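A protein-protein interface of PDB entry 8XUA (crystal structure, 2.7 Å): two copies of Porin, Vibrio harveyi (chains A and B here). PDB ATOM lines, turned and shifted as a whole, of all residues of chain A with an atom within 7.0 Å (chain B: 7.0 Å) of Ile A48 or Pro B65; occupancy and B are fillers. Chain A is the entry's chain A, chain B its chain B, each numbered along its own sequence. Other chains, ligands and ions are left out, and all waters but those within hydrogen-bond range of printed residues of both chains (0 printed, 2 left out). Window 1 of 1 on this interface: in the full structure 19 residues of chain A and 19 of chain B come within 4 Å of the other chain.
Of chain B, only Pro B65 (3.7 Å) comes within 4 Å of Ile A48. Of chain A, only Ile A48 and Gln A49 come within 4 Å of Pro B65. No residue of chain B comes within 4 Å of Gly A47. Of the printed residues of chain A, Ala B93 touches Leu A50 and Gly A51. Of the printed residues of chain B, Leu A50 touches Phe B45, Ile B67 and Ala B93. Of the printed residues of chain B, Ser A24 touches Phe B45. Printed residues of chain B within 4 Å of Gln A49: Pro B65 (3.3 Å). Printed residues of chain A within 4 Å of Gln B49: Pro A65 (3.2 Å). The nearest residue of chain B that does not touch Ile A48 is Ile B48 (4.05 Å). The nearest printed residue of chain B that does not touch Gly A51 is Ser B92 (5.6 Å).
Of the 18 printed residues of chain B, 9 touch a printed residue of chain A. Hydrophobic or aromatic side chains of chain B that line the printed part of chain A: Leu B26, Phe B45, Ile B48, Pro B65, Ile B67 and Ala B93. Hydrophobic or aromatic side chains of chain A that line the printed part of chain B: Leu A26, Phe A45, Ile A48, Leu A50 and Pro A65. Among the printed residues, no Asp or Glu carboxylate lies within 4 Å of a Lys or Arg side-chain nitrogen of the other chain.
N of Gly A51 sits at hydrogen-bond distance from OG of Ser A20 (3.0 Å). The backbone carbonyl oxygen of Ser A24 is in hydrogen-bond range of the backbone NH of Gly A47 (3.4 Å). N of Phe B45 lies within hydrogen-bond range of O of Leu B26 (2.8 Å). The side-chain amide oxygen of Gln B49 sits at hydrogen-bond distance from the backbone NH of Thr B63 (3.1 Å). O of Pro B65 lies within hydrogen-bond range of OG of Ser B92 (3.1 Å). O of Ile B67 is in hydrogen-bond range of N of Phe B91.
OD1 of Asn A62 sits close to O of Thr B63, at 3.4 Å. The backbone carbonyl oxygen (O) of Ala B93 lies close to the backbone carbonyl oxygen (O) of Gly A51 (3.4 Å).
Leu A26 touches its own counterpart, Leu B26. Leu A26 touches Phe B45, and with the chains exchanged Phe A45 touches Leu B26. Ile A48 touches Pro B65, and with the chains exchanged Pro A65 touches Ile B48. Gln A49 touches Pro B65, and with the chains exchanged Pro A65 touches Gln B49.
Among the printed residues, pairs that only touch across the chains: Ser A24 with Phe B45 (3.5 Å), Leu A26 with Leu B26 (3.6 Å), Leu A26 with Phe B45 (3.9 Å), Phe A45 with Leu B26 (3.9 Å), Ile A48 with Pro B65 (3.7 Å), Gln A49 with Pro B65 (3.3 Å), Leu A50 with Phe B45 (3.9 Å), Leu A50 with Ile B67 (3.6 Å), Leu A50 with Ala B93 (3.7 Å), Asn A62 with Thr B64 (3.9 Å), Pro A65 with Ile B48 (3.8 Å) and Pro A65 with Gln B49 (3.2 Å).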
ATOM      1  N   HIS A  18      22.961  21.524  -1.333  1.00  0.00           N
ATOM      2  CA  HIS A  18      22.759  20.571  -2.409  1.00  0.00           C
ATOM      3  C   HIS A  18      21.561  19.678  -2.207  1.00  0.00           C
ATOM      4  O   HIS A  18      21.155  19.019  -3.162  1.00  0.00           O
ATOM      5  CB  HIS A  18      23.986  19.693  -2.578  1.00  0.00           C
ATOM      6  CG  HIS A  18      25.233  20.469  -2.797  1.00  0.00           C
ATOM      7  ND1 HIS A  18      25.382  21.327  -3.862  1.00  0.00           N
ATOM      8  CD2 HIS A  18      26.390  20.524  -2.096  1.00  0.00           C
ATOM      9  CE1 HIS A  18      26.577  21.882  -3.809  1.00  0.00           C
ATOM     10  NE2 HIS A  18      27.210  21.412  -2.752  1.00  0.00           N
ATOM     11  N   SER A  20      21.674  16.997  -0.312  1.00  0.00           N
ATOM     12  CA  SER A  20      22.167  15.626  -0.291  1.00  0.00           C
ATOM     13  C   SER A  20      23.638  15.630   0.116  1.00  0.00           C
ATOM     14  O   SER A  20      24.338  16.618  -0.101  1.00  0.00           O
ATOM     15  CB  SER A  20      21.960  14.976  -1.666  1.00  0.00           C
ATOM     16  OG  SER A  20      22.651  13.763  -1.812  1.00  0.00           O
ATOM     17  N   MET A  22      25.950  13.584  -0.988  1.00  0.00           N
ATOM     18  CA  MET A  22      26.762  13.194  -2.117  1.00  0.00           C
ATOM     19  C   MET A  22      26.077  13.698  -3.377  1.00  0.00           C
ATOM     20  O   MET A  22      24.857  13.592  -3.504  1.00  0.00           O
ATOM     21  CB  MET A  22      26.936  11.672  -2.131  1.00  0.00           C
ATOM     22  CG  MET A  22      28.267  11.189  -2.654  1.00  0.00           C
ATOM     23  SD  MET A  22      28.390   9.407  -2.484  1.00  0.00           S
ATOM     24  CE  MET A  22      27.858   9.307  -0.753  1.00  0.00           C
ATOM     25  N   THR A  23      26.850  14.284  -4.287  1.00  0.00           N
ATOM     26  CA  THR A  23      26.314  14.677  -5.583  1.00  0.00           C
ATOM     27  C   THR A  23      27.345  14.423  -6.673  1.00  0.00           C
ATOM     28  O   THR A  23      28.516  14.149  -6.413  1.00  0.00           O
ATOM     29  CB  THR A  23      25.899  16.151  -5.626  1.00  0.00           C
ATOM     30  OG1 THR A  23      27.051  16.964  -5.385  1.00  0.00           O
ATOM     31  CG2 THR A  23      24.819  16.484  -4.591  1.00  0.00           C
ATOM     32  N   SER A  24      26.894  14.550  -7.908  1.00  0.00           N
ATOM     33  CA  SER A  24      27.718  14.468  -9.102  1.00  0.00           C
ATOM     34  C   SER A  24      27.350  15.599 -10.059  1.00  0.00           C
ATOM     35  O   SER A  24      26.179  15.987 -10.173  1.00  0.00           O
ATOM     36  CB  SER A  24      27.530  13.118  -9.806  1.00  0.00           C
ATOM     37  OG  SER A  24      28.102  13.130 -11.103  1.00  0.00           O
ATOM     38  N   THR A  25      28.355  16.117 -10.753  1.00  0.00           N
ATOM     39  CA  THR A  25      28.164  17.026 -11.872  1.00  0.00           C
ATOM     40  C   THR A  25      28.854  16.438 -13.092  1.00  0.00           C
ATOM     41  O   THR A  25      29.989  15.950 -12.998  1.00  0.00           O
ATOM     42  CB  THR A  25      28.731  18.394 -11.564  1.00  0.00           C
ATOM     43  OG1 THR A  25      28.171  18.846 -10.334  1.00  0.00           O
ATOM     44  CG2 THR A  25      28.365  19.371 -12.659  1.00  0.00           C
ATOM     45  N   LEU A  26      28.177  16.477 -14.234  1.00  0.00           N
ATOM     46  CA  LEU A  26      28.662  15.778 -15.412  1.00  0.00           C
ATOM     47  C   LEU A  26      28.476  16.684 -16.603  1.00  0.00           C
ATOM     48  O   LEU A  26      27.517  17.456 -16.658  1.00  0.00           O
ATOM     49  CB  LEU A  26      27.922  14.461 -15.657  1.00  0.00           C
ATOM     50  CG  LEU A  26      27.835  13.464 -14.503  1.00  0.00           C
ATOM     51  CD1 LEU A  26      26.858  12.362 -14.873  1.00  0.00           C
ATOM     52  CD2 LEU A  26      29.217  12.892 -14.155  1.00  0.00           C
ATOM     53  N   PHE A  45      24.858  18.409 -16.407  1.00  0.00           N
ATOM     54  CA  PHE A  45      23.942  18.029 -15.339  1.00  0.00           C
ATOM     55  C   PHE A  45      24.667  18.397 -14.050  1.00  0.00           C
ATOM     56  O   PHE A  45      25.678  17.779 -13.688  1.00  0.00           O
ATOM     57  CB  PHE A  45      23.577  16.543 -15.359  1.00  0.00           C
ATOM     58  CG  PHE A  45      22.877  16.082 -16.621  1.00  0.00           C
ATOM     59  CD1 PHE A  45      22.352  16.994 -17.522  1.00  0.00           C
ATOM     60  CD2 PHE A  45      22.755  14.720 -16.904  1.00  0.00           C
ATOM     61  CE1 PHE A  45      21.729  16.572 -18.652  1.00  0.00           C
ATOM     62  CE2 PHE A  45      22.125  14.277 -18.047  1.00  0.00           C
ATOM     63  CZ  PHE A  45      21.606  15.192 -18.921  1.00  0.00           C
ATOM     64  N   ASP A  46      24.176  19.427 -13.383  1.00  0.00           N
ATOM     65  CA  ASP A  46      24.713  19.855 -12.111  1.00  0.00           C
ATOM     66  C   ASP A  46      23.732  19.461 -11.009  1.00  0.00           C
ATOM     67  O   ASP A  46      22.526  19.687 -11.137  1.00  0.00           O
ATOM     68  CB  ASP A  46      24.948  21.360 -12.141  1.00  0.00           C
ATOM     69  CG  ASP A  46      25.652  21.853 -10.931  1.00  0.00           C
ATOM     70  OD1 ASP A  46      26.464  21.076 -10.384  1.00  0.00           O
ATOM     71  OD2 ASP A  46      25.349  22.991 -10.498  1.00  0.00           O
ATOM     72  N   GLY A  47      24.242  18.828  -9.959  1.00  0.00           N
ATOM     73  CA  GLY A  47      23.453  18.587  -8.775  1.00  0.00           C
ATOM     74  C   GLY A  47      22.737  17.262  -8.737  1.00  0.00           C
ATOM     75  O   GLY A  47      21.676  17.166  -8.102  1.00  0.00           O
ATOM     76  N   ILE A  48      23.257  16.242  -9.423  1.00  0.00           N
ATOM     77  CA  ILE A  48      22.644  14.922  -9.362  1.00  0.00           C
ATOM     78  C   ILE A  48      22.801  14.391  -7.944  1.00  0.00           C
ATOM     79  O   ILE A  48      23.920  14.218  -7.454  1.00  0.00           O
ATOM     80  CB  ILE A  48      23.282  13.970 -10.378  1.00  0.00           C
ATOM     81  CG1 ILE A  48      23.308  14.620 -11.767  1.00  0.00           C
ATOM     82  CG2 ILE A  48      22.538  12.608 -10.377  1.00  0.00           C
ATOM     83  CD1 ILE A  48      24.116  13.823 -12.801  1.00  0.00           C
ATOM     84  N   GLN A  49      21.687  14.138  -7.272  1.00  0.00           N
ATOM     85  CA  GLN A  49      21.771  13.729  -5.878  1.00  0.00           C
ATOM     86  C   GLN A  49      22.070  12.235  -5.774  1.00  0.00           C
ATOM     87  O   GLN A  49      21.327  11.410  -6.317  1.00  0.00           O
ATOM     88  CB  GLN A  49      20.488  14.098  -5.151  1.00  0.00           C
ATOM     89  CG  GLN A  49      20.292  15.578  -5.046  1.00  0.00           C
ATOM     90  CD  GLN A  49      19.056  15.910  -4.263  1.00  0.00           C
ATOM     91  OE1 GLN A  49      17.985  15.388  -4.550  1.00  0.00           O
ATOM     92  NE2 GLN A  49      19.185  16.785  -3.286  1.00  0.00           N
ATOM     93  N   LEU A  50      23.168  11.898  -5.085  1.00  0.00           N
ATOM     94  CA  LEU A  50      23.591  10.518  -4.870  1.00  0.00           C
ATOM     95  C   LEU A  50      23.500  10.073  -3.416  1.00  0.00           C
ATOM     96  O   LEU A  50      23.377   8.874  -3.165  1.00  0.00           O
ATOM     97  CB  LEU A  50      25.042  10.311  -5.351  1.00  0.00           C
ATOM     98  CG  LEU A  50      25.479  10.778  -6.760  1.00  0.00           C
ATOM     99  CD1 LEU A  50      26.900  10.355  -7.139  1.00  0.00           C
ATOM    100  CD2 LEU A  50      24.513  10.317  -7.834  1.00  0.00           C
ATOM    101  N   GLY A  51      23.555  11.000  -2.458  1.00  0.00           N
ATOM    102  CA  GLY A  51      23.639  10.671  -1.055  1.00  0.00           C
ATOM    103  C   GLY A  51      22.347  10.880  -0.272  1.00  0.00           C
ATOM    104  O   GLY A  51      21.291  11.248  -0.793  1.00  0.00           O
ATOM    105  N   ASN A  62      14.789  16.889  -1.650  1.00  0.00           N
ATOM    106  CA  ASN A  62      14.800  16.201  -2.936  1.00  0.00           C
ATOM    107  C   ASN A  62      14.651  17.236  -4.056  1.00  0.00           C
ATOM    108  O   ASN A  62      13.549  17.691  -4.362  1.00  0.00           O
ATOM    109  CB  ASN A  62      13.702  15.146  -2.977  1.00  0.00           C
ATOM    110  CG  ASN A  62      13.632  14.409  -4.315  1.00  0.00           C
ATOM    111  OD1 ASN A  62      14.463  14.605  -5.207  1.00  0.00           O
ATOM    112  ND2 ASN A  62      12.620  13.552  -4.457  1.00  0.00           N
ATOM    113  N   THR A  63      15.768  17.598  -4.678  1.00  0.00           N
ATOM    114  CA  THR A  63      15.793  18.545  -5.781  1.00  0.00           C
ATOM    115  C   THR A  63      15.599  17.819  -7.108  1.00  0.00           C
ATOM    116  O   THR A  63      15.559  16.584  -7.174  1.00  0.00           O
ATOM    117  CB  THR A  63      17.117  19.314  -5.821  1.00  0.00           C
ATOM    118  OG1 THR A  63      18.168  18.393  -6.142  1.00  0.00           O
ATOM    119  CG2 THR A  63      17.428  19.968  -4.471  1.00  0.00           C
ATOM    120  N   THR A  64      15.442  18.631  -8.196  1.00  0.00           N
ATOM    121  CA  THR A  64      15.636  18.157  -9.562  1.00  0.00           C
ATOM    122  C   THR A  64      16.911  18.775 -10.116  1.00  0.00           C
ATOM    123  O   THR A  64      17.244  19.909  -9.781  1.00  0.00           O
ATOM    124  CB  THR A  64      14.471  18.494 -10.501  1.00  0.00           C
ATOM    125  OG1 THR A  64      14.085  19.856 -10.324  1.00  0.00           O
ATOM    126  CG2 THR A  64      13.307  17.581 -10.267  1.00  0.00           C
ATOM    127  N   PRO A  65      17.654  18.059 -10.947  1.00  0.00           N
ATOM    128  CA  PRO A  65      18.995  18.524 -11.324  1.00  0.00           C
ATOM    129  C   PRO A  65      18.965  19.835 -12.113  1.00  0.00           C
ATOM    130  O   PRO A  65      17.950  20.224 -12.693  1.00  0.00           O
ATOM    131  CB  PRO A  65      19.535  17.384 -12.193  1.00  0.00           C
ATOM    132  CG  PRO A  65      18.517  16.329 -12.190  1.00  0.00           C
ATOM    133  CD  PRO A  65      17.236  16.875 -11.708  1.00  0.00           C
ATOM    134  N   ALA A  66      20.114  20.504 -12.151  1.00  0.00           N
ATOM    135  CA  ALA A  66      20.279  21.769 -12.862  1.00  0.00           C
ATOM    136  C   ALA A  66      20.844  21.482 -14.247  1.00  0.00           C
ATOM    137  O   ALA A  66      22.018  21.131 -14.373  1.00  0.00           O
ATOM    138  CB  ALA A  66      21.208  22.710 -12.092  1.00  0.00           C
ATOM    139  N   ILE A  67      20.030  21.646 -15.286  1.00  0.00           N
ATOM    140  CA  ILE A  67      20.418  21.304 -16.656  1.00  0.00           C
ATOM    141  C   ILE A  67      20.838  22.564 -17.406  1.00  0.00           C
ATOM    142  O   ILE A  67      20.046  23.499 -17.569  1.00  0.00           O
ATOM    143  CB  ILE A  67      19.284  20.599 -17.411  1.00  0.00           C
ATOM    144  CG1 ILE A  67      18.491  19.675 -16.490  1.00  0.00           C
ATOM    145  CG2 ILE A  67      19.860  19.847 -18.591  1.00  0.00           C
ATOM    146  CD1 ILE A  67      19.303  18.595 -15.825  1.00  0.00           C
ATOM    147  N   LEU B  26      23.141   7.536 -18.015  1.00  0.00           N
ATOM    148  CA  LEU B  26      24.544   7.692 -18.371  1.00  0.00           C
ATOM    149  C   LEU B  26      25.341   6.560 -17.749  1.00  0.00           C
ATOM    150  O   LEU B  26      25.062   6.129 -16.626  1.00  0.00           O
ATOM    151  CB  LEU B  26      25.104   9.045 -17.901  1.00  0.00           C
ATOM    152  CG  LEU B  26      24.331  10.283 -18.381  1.00  0.00           C
ATOM    153  CD1 LEU B  26      24.813  11.530 -17.680  1.00  0.00           C
ATOM    154  CD2 LEU B  26      24.406  10.487 -19.922  1.00  0.00           C
ATOM    155  N   GLU B  44      26.296   3.299 -13.531  1.00  0.00           N
ATOM    156  CA  GLU B  44      25.182   3.779 -14.338  1.00  0.00           C
ATOM    157  C   GLU B  44      24.373   4.720 -13.466  1.00  0.00           C
ATOM    158  O   GLU B  44      24.031   4.365 -12.331  1.00  0.00           O
ATOM    159  CB  GLU B  44      24.299   2.618 -14.831  1.00  0.00           C
ATOM    160  CG  GLU B  44      23.219   2.991 -15.822  1.00  0.00           C
ATOM    161  CD  GLU B  44      22.042   1.998 -15.824  1.00  0.00           C
ATOM    162  OE1 GLU B  44      21.409   1.849 -14.752  1.00  0.00           O
ATOM    163  OE2 GLU B  44      21.711   1.402 -16.887  1.00  0.00           O
ATOM    164  N   PHE B  45      24.125   5.929 -13.960  1.00  0.00           N
ATOM    165  CA  PHE B  45      23.181   6.850 -13.338  1.00  0.00           C
ATOM    166  C   PHE B  45      21.916   6.749 -14.155  1.00  0.00           C
ATOM    167  O   PHE B  45      21.881   7.203 -15.303  1.00  0.00           O
ATOM    168  CB  PHE B  45      23.689   8.290 -13.321  1.00  0.00           C
ATOM    169  CG  PHE B  45      24.887   8.517 -12.424  1.00  0.00           C
ATOM    170  CD1 PHE B  45      25.403   7.488 -11.640  1.00  0.00           C
ATOM    171  CD2 PHE B  45      25.478   9.776 -12.339  1.00  0.00           C
ATOM    172  CE1 PHE B  45      26.492   7.704 -10.821  1.00  0.00           C
ATOM    173  CE2 PHE B  45      26.567  10.000 -11.519  1.00  0.00           C
ATOM    174  CZ  PHE B  45      27.075   8.970 -10.751  1.00  0.00           C
ATOM    175  N   ASP B  46      20.886   6.133 -13.592  1.00  0.00           N
ATOM    176  CA  ASP B  46      19.653   5.889 -14.318  1.00  0.00           C
ATOM    177  C   ASP B  46      18.509   6.720 -13.749  1.00  0.00           C
ATOM    178  O   ASP B  46      18.356   6.849 -12.530  1.00  0.00           O
ATOM    179  CB  ASP B  46      19.311   4.409 -14.276  1.00  0.00           C
ATOM    180  CG  ASP B  46      18.160   4.041 -15.201  1.00  0.00           C
ATOM    181  OD1 ASP B  46      17.853   4.826 -16.130  1.00  0.00           O
ATOM    182  OD2 ASP B  46      17.572   2.959 -14.996  1.00  0.00           O
ATOM    183  N   GLY B  47      17.681   7.254 -14.639  1.00  0.00           N
ATOM    184  CA  GLY B  47      16.490   7.948 -14.218  1.00  0.00           C
ATOM    185  C   GLY B  47      16.686   9.412 -13.904  1.00  0.00           C
ATOM    186  O   GLY B  47      15.849  10.000 -13.206  1.00  0.00           O
ATOM    187  N   ILE B  48      17.776  10.024 -14.373  1.00  0.00           N
ATOM    188  CA  ILE B  48      17.968  11.447 -14.127  1.00  0.00           C
ATOM    189  C   ILE B  48      16.814  12.188 -14.781  1.00  0.00           C
ATOM    190  O   ILE B  48      16.463  11.923 -15.934  1.00  0.00           O
ATOM    191  CB  ILE B  48      19.328  11.910 -14.669  1.00  0.00           C
ATOM    192  CG1 ILE B  48      20.450  11.004 -14.165  1.00  0.00           C
ATOM    193  CG2 ILE B  48      19.615  13.304 -14.224  1.00  0.00           C
ATOM    194  CD1 ILE B  48      21.775  11.247 -14.863  1.00  0.00           C
ATOM    195  N   GLN B  49      16.189  13.091 -14.043  1.00  0.00           N
ATOM    196  CA  GLN B  49      14.965  13.727 -14.499  1.00  0.00           C
ATOM    197  C   GLN B  49      15.262  15.090 -15.105  1.00  0.00           C
ATOM    198  O   GLN B  49      15.896  15.930 -14.463  1.00  0.00           O
ATOM    199  CB  GLN B  49      13.986  13.836 -13.332  1.00  0.00           C
ATOM    200  CG  GLN B  49      13.510  12.500 -12.870  1.00  0.00           C
ATOM    201  CD  GLN B  49      12.327  12.577 -11.908  1.00  0.00           C
ATOM    202  OE1 GLN B  49      12.397  13.237 -10.880  1.00  0.00           O
ATOM    203  NE2 GLN B  49      11.255  11.864 -12.225  1.00  0.00           N
ATOM    204  N   THR B  63      11.799  11.902  -8.165  1.00  0.00           N
ATOM    205  CA  THR B  63      12.502  10.727  -7.671  1.00  0.00           C
ATOM    206  C   THR B  63      13.947  11.077  -7.345  1.00  0.00           C
ATOM    207  O   THR B  63      14.407  12.208  -7.553  1.00  0.00           O
ATOM    208  CB  THR B  63      12.467   9.604  -8.703  1.00  0.00           C
ATOM    209  OG1 THR B  63      13.120  10.063  -9.891  1.00  0.00           O
ATOM    210  CG2 THR B  63      11.055   9.231  -9.046  1.00  0.00           C
ATOM    211  N   THR B  64      14.663  10.081  -6.787  1.00  0.00           N
ATOM    212  CA  THR B  64      16.105  10.218  -6.755  1.00  0.00           C
ATOM    213  C   THR B  64      16.731   9.182  -7.687  1.00  0.00           C
ATOM    214  O   THR B  64      16.207   8.078  -7.851  1.00  0.00           O
ATOM    215  CB  THR B  64      16.694  10.076  -5.344  1.00  0.00           C
ATOM    216  OG1 THR B  64      16.209   8.877  -4.715  1.00  0.00           O
ATOM    217  CG2 THR B  64      16.351  11.308  -4.501  1.00  0.00           C
ATOM    218  N   PRO B  65      17.821   9.527  -8.354  1.00  0.00           N
ATOM    219  CA  PRO B  65      18.309   8.666  -9.432  1.00  0.00           C
ATOM    220  C   PRO B  65      18.676   7.262  -8.946  1.00  0.00           C
ATOM    221  O   PRO B  65      19.030   7.025  -7.787  1.00  0.00           O
ATOM    222  CB  PRO B  65      19.547   9.409  -9.952  1.00  0.00           C
ATOM    223  CG  PRO B  65      19.590  10.687  -9.266  1.00  0.00           C
ATOM    224  CD  PRO B  65      18.699  10.680  -8.101  1.00  0.00           C
ATOM    225  N   ALA B  66      18.616   6.325  -9.877  1.00  0.00           N
ATOM    226  CA  ALA B  66      19.031   4.954  -9.640  1.00  0.00           C
ATOM    227  C   ALA B  66      20.523   4.826  -9.937  1.00  0.00           C
ATOM    228  O   ALA B  66      20.935   4.889 -11.100  1.00  0.00           O
ATOM    229  CB  ALA B  66      18.207   4.027 -10.525  1.00  0.00           C
ATOM    230  N   ILE B  67      21.336   4.617  -8.905  1.00  0.00           N
ATOM    231  CA  ILE B  67      22.775   4.446  -9.085  1.00  0.00           C
ATOM    232  C   ILE B  67      23.103   2.962  -9.021  1.00  0.00           C
ATOM    233  O   ILE B  67      22.895   2.325  -7.984  1.00  0.00           O
ATOM    234  CB  ILE B  67      23.579   5.218  -8.032  1.00  0.00           C
ATOM    235  CG1 ILE B  67      22.894   6.545  -7.659  1.00  0.00           C
ATOM    236  CG2 ILE B  67      24.992   5.452  -8.542  1.00  0.00           C
ATOM    237  CD1 ILE B  67      22.503   7.474  -8.839  1.00  0.00           C
ATOM    238  N   THR B  68      23.630   2.419 -10.119  1.00  0.00           N
ATOM    239  CA  THR B  68      24.137   1.055 -10.215  1.00  0.00           C
ATOM    240  C   THR B  68      25.667   1.053 -10.184  1.00  0.00           C
ATOM    241  O   THR B  68      26.304   1.859 -10.863  1.00  0.00           O
ATOM    242  CB  THR B  68      23.675   0.424 -11.526  1.00  0.00           C
ATOM    243  OG1 THR B  68      22.262   0.218 -11.492  1.00  0.00           O
ATOM    244  CG2 THR B  68      24.404  -0.877 -11.838  1.00  0.00           C
ATOM    245  N   LEU B  90      22.217  -1.685  -6.481  1.00  0.00           N
ATOM    246  CA  LEU B  90      21.418  -0.498  -6.725  1.00  0.00           C
ATOM    247  C   LEU B  90      21.398   0.350  -5.466  1.00  0.00           C
ATOM    248  O   LEU B  90      20.949  -0.117  -4.412  1.00  0.00           O
ATOM    249  CB  LEU B  90      20.001  -0.874  -7.148  1.00  0.00           C
ATOM    250  CG  LEU B  90      19.016   0.278  -7.426  1.00  0.00           C
ATOM    251  CD1 LEU B  90      19.535   1.301  -8.489  1.00  0.00           C
ATOM    252  CD2 LEU B  90      17.638  -0.275  -7.838  1.00  0.00           C
ATOM    253  N   PHE B  91      21.895   1.584  -5.571  1.00  0.00           N
ATOM    254  CA  PHE B  91      21.755   2.579  -4.518  1.00  0.00           C
ATOM    255  C   PHE B  91      20.808   3.694  -4.968  1.00  0.00           C
ATOM    256  O   PHE B  91      20.609   3.934  -6.161  1.00  0.00           O
ATOM    257  CB  PHE B  91      23.101   3.199  -4.138  1.00  0.00           C
ATOM    258  CG  PHE B  91      24.149   2.227  -3.650  1.00  0.00           C
ATOM    259  CD1 PHE B  91      24.164   1.798  -2.324  1.00  0.00           C
ATOM    260  CD2 PHE B  91      25.192   1.823  -4.498  1.00  0.00           C
ATOM    261  CE1 PHE B  91      25.166   0.925  -1.865  1.00  0.00           C
ATOM    262  CE2 PHE B  91      26.207   0.962  -4.054  1.00  0.00           C
ATOM    263  CZ  PHE B  91      26.192   0.507  -2.735  1.00  0.00           C
ATOM    264  N   SER B  92      20.229   4.399  -4.000  1.00  0.00           N
ATOM    265  CA  SER B  92      19.490   5.611  -4.329  1.00  0.00           C
ATOM    266  C   SER B  92      19.399   6.490  -3.103  1.00  0.00           C
ATOM    267  O   SER B  92      19.005   6.017  -2.036  1.00  0.00           O
ATOM    268  CB  SER B  92      18.090   5.326  -4.827  1.00  0.00           C
ATOM    269  OG  SER B  92      17.464   6.557  -5.185  1.00  0.00           O
ATOM    270  N   ALA B  93      19.724   7.770  -3.273  1.00  0.00           N
ATOM    271  CA  ALA B  93      19.694   8.746  -2.193  1.00  0.00           C
ATOM    272  C   ALA B  93      20.454   8.214  -0.974  1.00  0.00           C
ATOM    273  O   ALA B  93      19.974   8.229   0.163  1.00  0.00           O
ATOM    274  CB  ALA B  93      18.253   9.135  -1.858  1.00  0.00           C
ATOM    275  N   ILE B  97      19.336  -0.104  -2.280  1.00  0.00           N
ATOM    276  CA  ILE B  97      18.001  -0.370  -2.775  1.00  0.00           C
ATOM    277  C   ILE B  97      17.809  -1.836  -3.114  1.00  0.00           C
ATOM    278  O   ILE B  97      16.829  -2.446  -2.693  1.00  0.00           O
ATOM    279  CB  ILE B  97      17.688   0.540  -3.982  1.00  0.00           C
ATOM    280  CG1 ILE B  97      17.870   2.009  -3.592  1.00  0.00           C
ATOM    281  CG2 ILE B  97      16.246   0.347  -4.430  1.00  0.00           C
ATOM    282  CD1 ILE B  97      17.037   2.431  -2.393  1.00  0.00           C
